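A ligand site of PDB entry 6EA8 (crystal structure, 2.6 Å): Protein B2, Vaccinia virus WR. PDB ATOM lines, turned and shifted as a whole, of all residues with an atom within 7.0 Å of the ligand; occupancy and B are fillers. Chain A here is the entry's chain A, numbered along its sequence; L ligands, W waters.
The backbone carbonyl oxygen (O) of Val 131 lies within hydrogen-bond range of the guanidinium group (NH2) of Arg 183, 2.9 Å away.
NE of Arg 183 is in salt-bridge range of OE2 of Glu 180 (2.9 Å).
The guanidinium group (NH2) of Arg 183 sits at hydrogen-bond distance from the side-chain amide oxygen (OE1) of Gln 170 (2.5 Å).
A nitrogen (N4) of the ligand is in hydrogen-bond range of the guanidinium group (NH1) of Arg 185 (3.1 Å).
NZ of Lys 143 sits at hydrogen-bond distance from N7 of the ligand (3.0 Å).
The side-chain amino group (NZ) of Lys 187 is in hydrogen-bond range of an oxygen (O4) of the ligand (2.7 Å).
O11 of the ligand sits at hydrogen-bond distance from OH of Tyr 139, 2.7 Å away.
S1 of the ligand sits close to NH2 of Arg 183 (3.5 Å).
A nitrogen (N8) of the ligand is in hydrogen-bond range of the side-chain amide nitrogen (ND2) of Asn 150, at 3.2 Å.
A sulfur (S1) of the ligand sits close to the backbone NH (N) of Val 131, at 2.8 Å.
O of Val 131 lies close to S1 of the ligand.
The side-chain amide nitrogen of Gln 170 sits close to a sulfur (S1) of the ligand, at 2.6 Å.
Water W2 bridges an oxygen (O8) of the ligand (2.5 Å) and the side-chain amino group of Lys 143 (2.7 Å).
Water W1 lies within hydrogen-bond range of the side-chain amino group of Lys 187 and a nitrogen (N5) of the ligand.
Residues that only touch the ligand: Ala 146 (3.5 Å), Ala 130 (3.6 Å) and Ile 168 (3.9 Å).
Hydrophobic or aromatic side chains within 4 Å of the ligand: Ala 130, Val 131, Tyr 139, Ala 146 and Ile 168.
11 residues have an atom within 4 Å of the ligand: Ala 130, Val 131, Tyr 139, Lys 143, Ala 146, Asn 150, Ile 168, Gln 170, Arg 183, Arg 185 and Lys 187.
The nearest printed residue that does not touch the ligand is Tyr 132 (4.1 Å).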
ATOM      1  N   LEU A 125     -12.536 -16.005  -6.958  1.00  0.00           N
ATOM      2  CA  LEU A 125     -12.717 -15.332  -8.240  1.00  0.00           C
ATOM      3  C   LEU A 125     -14.094 -14.674  -8.267  1.00  0.00           C
ATOM      4  O   LEU A 125     -15.112 -15.366  -8.350  1.00  0.00           O
ATOM      5  CB  LEU A 125     -12.553 -16.329  -9.389  1.00  0.00           C
ATOM      6  CG  LEU A 125     -12.780 -15.759 -10.786  1.00  0.00           C
ATOM      7  CD1 LEU A 125     -11.871 -14.563 -11.030  1.00  0.00           C
ATOM      8  CD2 LEU A 125     -12.569 -16.832 -11.844  1.00  0.00           C
ATOM      9  N   GLY A 128     -17.850 -12.694 -13.034  1.00  0.00           N
ATOM     10  CA  GLY A 128     -17.695 -11.764 -14.132  1.00  0.00           C
ATOM     11  C   GLY A 128     -16.266 -11.348 -14.418  1.00  0.00           C
ATOM     12  O   GLY A 128     -16.020 -10.705 -15.440  1.00  0.00           O
ATOM     13  N   ASN A 129     -15.317 -11.698 -13.554  1.00  0.00           N
ATOM     14  CA  ASN A 129     -13.924 -11.306 -13.729  1.00  0.00           C
ATOM     15  C   ASN A 129     -13.175 -12.315 -14.588  1.00  0.00           C
ATOM     16  O   ASN A 129     -13.397 -13.522 -14.505  1.00  0.00           O
ATOM     17  CB  ASN A 129     -13.232 -11.173 -12.376  1.00  0.00           C
ATOM     18  CG  ASN A 129     -13.228  -9.743 -11.861  1.00  0.00           C
ATOM     19  OD1 ASN A 129     -13.993  -8.895 -12.334  1.00  0.00           O
ATOM     20  ND2 ASN A 129     -12.360  -9.464 -10.892  1.00  0.00           N
ATOM     21  N   ALA A 130     -12.289 -11.789 -15.431  1.00  0.00           N
ATOM     22  CA  ALA A 130     -11.324 -12.614 -16.141  1.00  0.00           C
ATOM     23  C   ALA A 130     -10.042 -12.728 -15.327  1.00  0.00           C
ATOM     24  O   ALA A 130      -9.857 -12.036 -14.317  1.00  0.00           O
ATOM     25  CB  ALA A 130     -11.032 -12.026 -17.524  1.00  0.00           C
ATOM     26  N   VAL A 131      -9.145 -13.604 -15.766  1.00  0.00           N
ATOM     27  CA  VAL A 131      -7.923 -13.898 -15.031  1.00  0.00           C
ATOM     28  C   VAL A 131      -6.743 -13.875 -15.987  1.00  0.00           C
ATOM     29  O   VAL A 131      -6.762 -14.543 -17.026  1.00  0.00           O
ATOM     30  CB  VAL A 131      -7.996 -15.277 -14.323  1.00  0.00           C
ATOM     31  CG1 VAL A 131      -6.625 -15.684 -13.799  1.00  0.00           C
ATOM     32  CG2 VAL A 131      -9.012 -15.239 -13.197  1.00  0.00           C
ATOM     33  N   TYR A 132      -5.721 -13.089 -15.639  1.00  0.00           N
ATOM     34  CA  TYR A 132      -4.409 -13.197 -16.258  1.00  0.00           C
ATOM     35  C   TYR A 132      -3.354 -13.190 -15.167  1.00  0.00           C
ATOM     36  O   TYR A 132      -3.331 -12.283 -14.328  1.00  0.00           O
ATOM     37  CB  TYR A 132      -4.125 -12.065 -17.249  1.00  0.00           C
ATOM     38  CG  TYR A 132      -2.751 -12.184 -17.879  1.00  0.00           C
ATOM     39  CD1 TYR A 132      -1.638 -11.583 -17.303  1.00  0.00           C
ATOM     40  CD2 TYR A 132      -2.564 -12.933 -19.042  1.00  0.00           C
ATOM     41  CE1 TYR A 132      -0.377 -11.703 -17.873  1.00  0.00           C
ATOM     42  CE2 TYR A 132      -1.315 -13.056 -19.617  1.00  0.00           C
ATOM     43  CZ  TYR A 132      -0.225 -12.438 -19.035  1.00  0.00           C
ATOM     44  OH  TYR A 132       1.014 -12.566 -19.601  1.00  0.00           O
ATOM     45  N   TYR A 139     -12.875  -8.158 -18.319  1.00  0.00           N
ATOM     46  CA  TYR A 139     -12.304  -8.749 -19.521  1.00  0.00           C
ATOM     47  C   TYR A 139     -11.405  -7.766 -20.261  1.00  0.00           C
ATOM     48  O   TYR A 139     -10.289  -8.117 -20.672  1.00  0.00           O
ATOM     49  CB  TYR A 139     -13.417  -9.256 -20.445  1.00  0.00           C
ATOM     50  CG  TYR A 139     -12.909  -9.823 -21.749  1.00  0.00           C
ATOM     51  CD1 TYR A 139     -12.440 -11.117 -21.830  1.00  0.00           C
ATOM     52  CD2 TYR A 139     -12.902  -9.044 -22.903  1.00  0.00           C
ATOM     53  CE1 TYR A 139     -11.970 -11.630 -23.020  1.00  0.00           C
ATOM     54  CE2 TYR A 139     -12.434  -9.555 -24.107  1.00  0.00           C
ATOM     55  CZ  TYR A 139     -11.972 -10.858 -24.152  1.00  0.00           C
ATOM     56  OH  TYR A 139     -11.502 -11.371 -25.342  1.00  0.00           O
ATOM     57  N   ILE A 142      -8.011  -7.299 -18.467  1.00  0.00           N
ATOM     58  CA  ILE A 142      -7.214  -8.531 -18.556  1.00  0.00           C
ATOM     59  C   ILE A 142      -6.719  -8.732 -19.975  1.00  0.00           C
ATOM     60  O   ILE A 142      -5.556  -9.083 -20.206  1.00  0.00           O
ATOM     61  CB  ILE A 142      -8.049  -9.724 -18.071  1.00  0.00           C
ATOM     62  CG1 ILE A 142      -8.300  -9.624 -16.566  1.00  0.00           C
ATOM     63  CG2 ILE A 142      -7.380 -11.032 -18.424  1.00  0.00           C
ATOM     64  CD1 ILE A 142      -7.043  -9.530 -15.727  1.00  0.00           C
ATOM     65  N   LYS A 143      -7.597  -8.498 -20.961  1.00  0.00           N
ATOM     66  CA  LYS A 143      -7.226  -8.679 -22.358  1.00  0.00           C
ATOM     67  C   LYS A 143      -6.081  -7.752 -22.754  1.00  0.00           C
ATOM     68  O   LYS A 143      -5.114  -8.187 -23.391  1.00  0.00           O
ATOM     69  CB  LYS A 143      -8.435  -8.443 -23.254  1.00  0.00           C
ATOM     70  CG  LYS A 143      -8.753  -9.627 -24.164  1.00  0.00           C
ATOM     71  CD  LYS A 143      -7.530 -10.094 -24.939  1.00  0.00           C
ATOM     72  CE  LYS A 143      -7.909 -10.937 -26.147  1.00  0.00           C
ATOM     73  NZ  LYS A 143      -6.752 -11.748 -26.619  1.00  0.00           N
ATOM     74  N   ALA A 146      -2.803  -8.910 -21.160  1.00  0.00           N
ATOM     75  CA  ALA A 146      -2.255 -10.082 -21.822  1.00  0.00           C
ATOM     76  C   ALA A 146      -1.502  -9.701 -23.096  1.00  0.00           C
ATOM     77  O   ALA A 146      -0.450 -10.268 -23.396  1.00  0.00           O
ATOM     78  CB  ALA A 146      -3.366 -11.078 -22.133  1.00  0.00           C
ATOM     79  N   LYS A 147      -2.039  -8.735 -23.842  1.00  0.00           N
ATOM     80  CA  LYS A 147      -1.332  -8.256 -25.023  1.00  0.00           C
ATOM     81  C   LYS A 147      -0.070  -7.491 -24.637  1.00  0.00           C
ATOM     82  O   LYS A 147       0.956  -7.592 -25.325  1.00  0.00           O
ATOM     83  CB  LYS A 147      -2.256  -7.369 -25.871  1.00  0.00           C
ATOM     84  CG  LYS A 147      -3.312  -8.149 -26.646  1.00  0.00           C
ATOM     85  CD  LYS A 147      -4.062  -7.244 -27.612  1.00  0.00           C
ATOM     86  CE  LYS A 147      -5.230  -6.540 -26.937  1.00  0.00           C
ATOM     87  NZ  LYS A 147      -6.524  -6.886 -27.601  1.00  0.00           N
ATOM     88  N   MET A 149       1.818  -7.894 -21.797  1.00  0.00           N
ATOM     89  CA  MET A 149       2.768  -8.897 -21.345  1.00  0.00           C
ATOM     90  C   MET A 149       3.186  -9.851 -22.449  1.00  0.00           C
ATOM     91  O   MET A 149       4.146 -10.606 -22.268  1.00  0.00           O
ATOM     92  CB  MET A 149       2.177  -9.693 -20.181  1.00  0.00           C
ATOM     93  CG  MET A 149       1.784  -8.848 -18.974  1.00  0.00           C
ATOM     94  SD  MET A 149       3.188  -7.995 -18.236  1.00  0.00           S
ATOM     95  CE  MET A 149       4.229  -9.384 -17.800  1.00  0.00           C
ATOM     96  N   ASN A 150       2.497  -9.837 -23.594  1.00  0.00           N
ATOM     97  CA  ASN A 150       2.798 -10.789 -24.665  1.00  0.00           C
ATOM     98  C   ASN A 150       4.170 -10.538 -25.274  1.00  0.00           C
ATOM     99  O   ASN A 150       4.837 -11.490 -25.709  1.00  0.00           O
ATOM    100  CB  ASN A 150       1.723 -10.717 -25.749  1.00  0.00           C
ATOM    101  CG  ASN A 150       1.424 -12.071 -26.366  1.00  0.00           C
ATOM    102  OD1 ASN A 150       2.164 -13.035 -26.171  1.00  0.00           O
ATOM    103  ND2 ASN A 150       0.337 -12.145 -27.136  1.00  0.00           N
ATOM    104  N   ILE A 168     -16.561 -21.298 -12.423  1.00  0.00           N
ATOM    105  CA  ILE A 168     -15.349 -21.796 -13.050  1.00  0.00           C
ATOM    106  C   ILE A 168     -14.212 -21.699 -12.047  1.00  0.00           C
ATOM    107  O   ILE A 168     -14.237 -20.883 -11.125  1.00  0.00           O
ATOM    108  CB  ILE A 168     -15.014 -21.016 -14.341  1.00  0.00           C
ATOM    109  CG1 ILE A 168     -13.906 -21.710 -15.136  1.00  0.00           C
ATOM    110  CG2 ILE A 168     -14.613 -19.573 -14.017  1.00  0.00           C
ATOM    111  CD1 ILE A 168     -13.588 -21.043 -16.477  1.00  0.00           C
ATOM    112  N   GLN A 170      -9.777 -21.761 -12.070  1.00  0.00           N
ATOM    113  CA  GLN A 170      -8.594 -21.653 -12.914  1.00  0.00           C
ATOM    114  C   GLN A 170      -7.336 -21.648 -12.051  1.00  0.00           C
ATOM    115  O   GLN A 170      -7.343 -21.151 -10.922  1.00  0.00           O
ATOM    116  CB  GLN A 170      -8.618 -20.386 -13.773  1.00  0.00           C
ATOM    117  CG  GLN A 170      -9.822 -20.243 -14.691  1.00  0.00           C
ATOM    118  CD  GLN A 170      -9.710 -19.030 -15.600  1.00  0.00           C
ATOM    119  OE1 GLN A 170      -8.853 -18.986 -16.495  1.00  0.00           O
ATOM    120  NE2 GLN A 170     -10.556 -18.040 -15.370  1.00  0.00           N
ATOM    121  N   LYS A 179       4.180 -12.312 -15.786  1.00  0.00           N
ATOM    122  CA  LYS A 179       3.674 -12.868 -17.030  1.00  0.00           C
ATOM    123  C   LYS A 179       3.120 -14.261 -16.796  1.00  0.00           C
ATOM    124  O   LYS A 179       3.722 -15.087 -16.106  1.00  0.00           O
ATOM    125  CB  LYS A 179       4.778 -12.924 -18.078  1.00  0.00           C
ATOM    126  CG  LYS A 179       4.280 -13.382 -19.440  1.00  0.00           C
ATOM    127  CD  LYS A 179       5.406 -13.519 -20.445  1.00  0.00           C
ATOM    128  CE  LYS A 179       4.863 -13.905 -21.811  1.00  0.00           C
ATOM    129  NZ  LYS A 179       5.935 -14.025 -22.827  1.00  0.00           N
ATOM    130  N   GLU A 180       1.961 -14.522 -17.399  1.00  0.00           N
ATOM    131  CA  GLU A 180       1.331 -15.831 -17.286  1.00  0.00           C
ATOM    132  C   GLU A 180       2.088 -16.847 -18.127  1.00  0.00           C
ATOM    133  O   GLU A 180       2.279 -16.651 -19.337  1.00  0.00           O
ATOM    134  CB  GLU A 180      -0.129 -15.748 -17.716  1.00  0.00           C
ATOM    135  CG  GLU A 180      -0.934 -17.012 -17.534  1.00  0.00           C
ATOM    136  CD  GLU A 180      -2.403 -16.797 -17.829  1.00  0.00           C
ATOM    137  OE1 GLU A 180      -3.044 -16.020 -17.097  1.00  0.00           O
ATOM    138  OE2 GLU A 180      -2.907 -17.395 -18.804  1.00  0.00           O
ATOM    139  N   ARG A 183      -1.791 -21.905 -17.756  1.00  0.00           N
ATOM    140  CA  ARG A 183      -3.160 -21.700 -17.289  1.00  0.00           C
ATOM    141  C   ARG A 183      -3.990 -22.951 -17.520  1.00  0.00           C
ATOM    142  O   ARG A 183      -4.030 -23.476 -18.638  1.00  0.00           O
ATOM    143  CB  ARG A 183      -3.813 -20.519 -18.002  1.00  0.00           C
ATOM    144  CG  ARG A 183      -5.270 -20.322 -17.601  1.00  0.00           C
ATOM    145  CD  ARG A 183      -6.067 -19.669 -18.709  1.00  0.00           C
ATOM    146  NE  ARG A 183      -5.657 -18.290 -18.929  1.00  0.00           N
ATOM    147  CZ  ARG A 183      -6.153 -17.246 -18.285  1.00  0.00           C
ATOM    148  NH1 ARG A 183      -5.733 -16.026 -18.557  1.00  0.00           N
ATOM    149  NH2 ARG A 183      -7.078 -17.428 -17.348  1.00  0.00           N
ATOM    150  N   ARG A 185      -8.011 -24.659 -16.665  1.00  0.00           N
ATOM    151  CA  ARG A 185      -9.389 -24.296 -16.348  1.00  0.00           C
ATOM    152  C   ARG A 185     -10.168 -25.543 -15.944  1.00  0.00           C
ATOM    153  O   ARG A 185     -10.126 -26.552 -16.648  1.00  0.00           O
ATOM    154  CB  ARG A 185     -10.091 -23.614 -17.525  1.00  0.00           C
ATOM    155  CG  ARG A 185      -9.513 -22.274 -17.928  1.00  0.00           C
ATOM    156  CD  ARG A 185     -10.368 -21.640 -19.023  1.00  0.00           C
ATOM    157  NE  ARG A 185      -9.709 -20.511 -19.647  1.00  0.00           N
ATOM    158  CZ  ARG A 185      -9.031 -20.579 -20.796  1.00  0.00           C
ATOM    159  NH1 ARG A 185      -8.930 -21.735 -21.436  1.00  0.00           N
ATOM    160  NH2 ARG A 185      -8.465 -19.494 -21.297  1.00  0.00           N
ATOM    161  N   LYS A 187     -14.058 -26.528 -15.352  1.00  0.00           N
ATOM    162  CA  LYS A 187     -15.395 -26.011 -15.649  1.00  0.00           C
ATOM    163  C   LYS A 187     -16.385 -26.498 -14.590  1.00  0.00           C
ATOM    164  O   LYS A 187     -17.330 -27.256 -14.860  1.00  0.00           O
ATOM    165  CB  LYS A 187     -15.811 -26.394 -17.057  1.00  0.00           C
ATOM    166  CG  LYS A 187     -14.822 -25.932 -18.119  1.00  0.00           C
ATOM    167  CD  LYS A 187     -14.322 -24.514 -17.865  1.00  0.00           C
ATOM    168  CE  LYS A 187     -13.463 -24.001 -19.015  1.00  0.00           C
ATOM    169  NZ  LYS A 187     -14.270 -23.618 -20.201  1.00  0.00           N
HETATM  170  C1  LIG L   1      -8.629 -14.982 -22.610  1.00  0.00           C
HETATM  171  C2  LIG L   1      -6.519 -14.042 -22.912  1.00  0.00           C
HETATM  172  C3  LIG L   1      -4.321 -13.855 -24.007  1.00  0.00           C
HETATM  173  C4  LIG L   1      -3.575 -12.767 -25.922  1.00  0.00           C
HETATM  174  C5  LIG L   1      -4.379 -15.057 -22.187  1.00  0.00           C
HETATM  175  C6  LIG L   1      -3.064 -14.335 -23.779  1.00  0.00           C
HETATM  176  C7  LIG L   1     -12.947 -18.912 -21.658  1.00  0.00           C
HETATM  177  C8  LIG L   1     -12.252 -21.313 -22.046  1.00  0.00           C
HETATM  178  C9  LIG L   1     -12.903 -14.770 -21.365  1.00  0.00           C
HETATM  179  C10 LIG L   1     -12.648 -16.072 -20.741  1.00  0.00           C
HETATM  180  C11 LIG L   1     -13.940 -16.779 -20.855  1.00  0.00           C
HETATM  181  C12 LIG L   1     -11.317 -19.566 -23.534  1.00  0.00           C
HETATM  182  C13 LIG L   1     -13.044 -20.231 -21.285  1.00  0.00           C
HETATM  183  C14 LIG L   1     -14.303 -19.048 -19.960  1.00  0.00           C
HETATM  184  C15 LIG L   1     -13.943 -15.054 -22.422  1.00  0.00           C
HETATM  185  C16 LIG L   1     -13.292 -15.085 -23.779  1.00  0.00           C
HETATM  186  C17 LIG L   1      -7.355 -15.212 -23.297  1.00  0.00           C
HETATM  187  C18 LIG L   1      -2.038 -13.979 -24.695  1.00  0.00           C
HETATM  188  C19 LIG L   1      -8.308 -14.069 -21.448  1.00  0.00           C
HETATM  189  C20 LIG L   1      -8.556 -14.814 -20.173  1.00  0.00           C
HETATM  190  N1  LIG L   1     -13.735 -18.188 -20.838  1.00  0.00           N
HETATM  191  N2  LIG L   1     -12.070 -18.552 -22.811  1.00  0.00           N
HETATM  192  N3  LIG L   1     -10.474 -19.193 -24.650  1.00  0.00           N
HETATM  193  N4  LIG L   1     -11.418 -20.946 -23.140  1.00  0.00           N
HETATM  194  N5  LIG L   1     -13.878 -20.307 -20.246  1.00  0.00           N
HETATM  195  N6  LIG L   1      -5.129 -14.318 -23.017  1.00  0.00           N
HETATM  196  N7  LIG L   1      -4.556 -13.068 -25.099  1.00  0.00           N
HETATM  197  N8  LIG L   1      -2.341 -13.203 -25.735  1.00  0.00           N
HETATM  198  N9  LIG L   1      -0.672 -14.441 -24.525  1.00  0.00           N
HETATM  199  N10 LIG L   1      -3.115 -15.080 -22.650  1.00  0.00           N
HETATM  200  O1  LIG L   1     -13.424 -13.861 -20.417  1.00  0.00           O
HETATM  201  O2  LIG L   1     -12.258 -15.935 -19.369  1.00  0.00           O
HETATM  202  O3  LIG L   1     -10.069 -17.077 -19.586  1.00  0.00           O
HETATM  203  O4  LIG L   1     -12.328 -22.445 -21.723  1.00  0.00           O
HETATM  204  O5  LIG L   1     -14.534 -16.332 -22.110  1.00  0.00           O
HETATM  205  O6  LIG L   1     -12.066 -15.754 -23.708  1.00  0.00           O
HETATM  206  O7  LIG L   1      -9.637 -14.347 -23.427  1.00  0.00           O
HETATM  207  O8  LIG L   1      -7.472 -15.294 -24.727  1.00  0.00           O
HETATM  208  O9  LIG L   1      -6.909 -13.745 -21.547  1.00  0.00           O
HETATM  209  O10 LIG L   1      -9.891 -14.623 -19.814  1.00  0.00           O
HETATM  210  O11 LIG L   1     -11.296 -14.094 -25.225  1.00  0.00           O
HETATM  211  P1  LIG L   1     -10.650 -15.852 -19.035  1.00  0.00           P
HETATM  212  P2  LIG L   1     -10.705 -15.153 -24.413  1.00  0.00           P
HETATM  213  S1  LIG L   1     -10.224 -15.953 -16.964  1.00  0.00           S
HETATM  214  S2  LIG L   1      -9.852 -16.502 -25.826  1.00  0.00           S
HETATM  215  O   HOH W   1     -16.416 -22.380 -19.054  1.00  0.00           O
HETATM  216  O   HOH W   2      -8.523 -13.782 -26.402  1.00  0.00           O
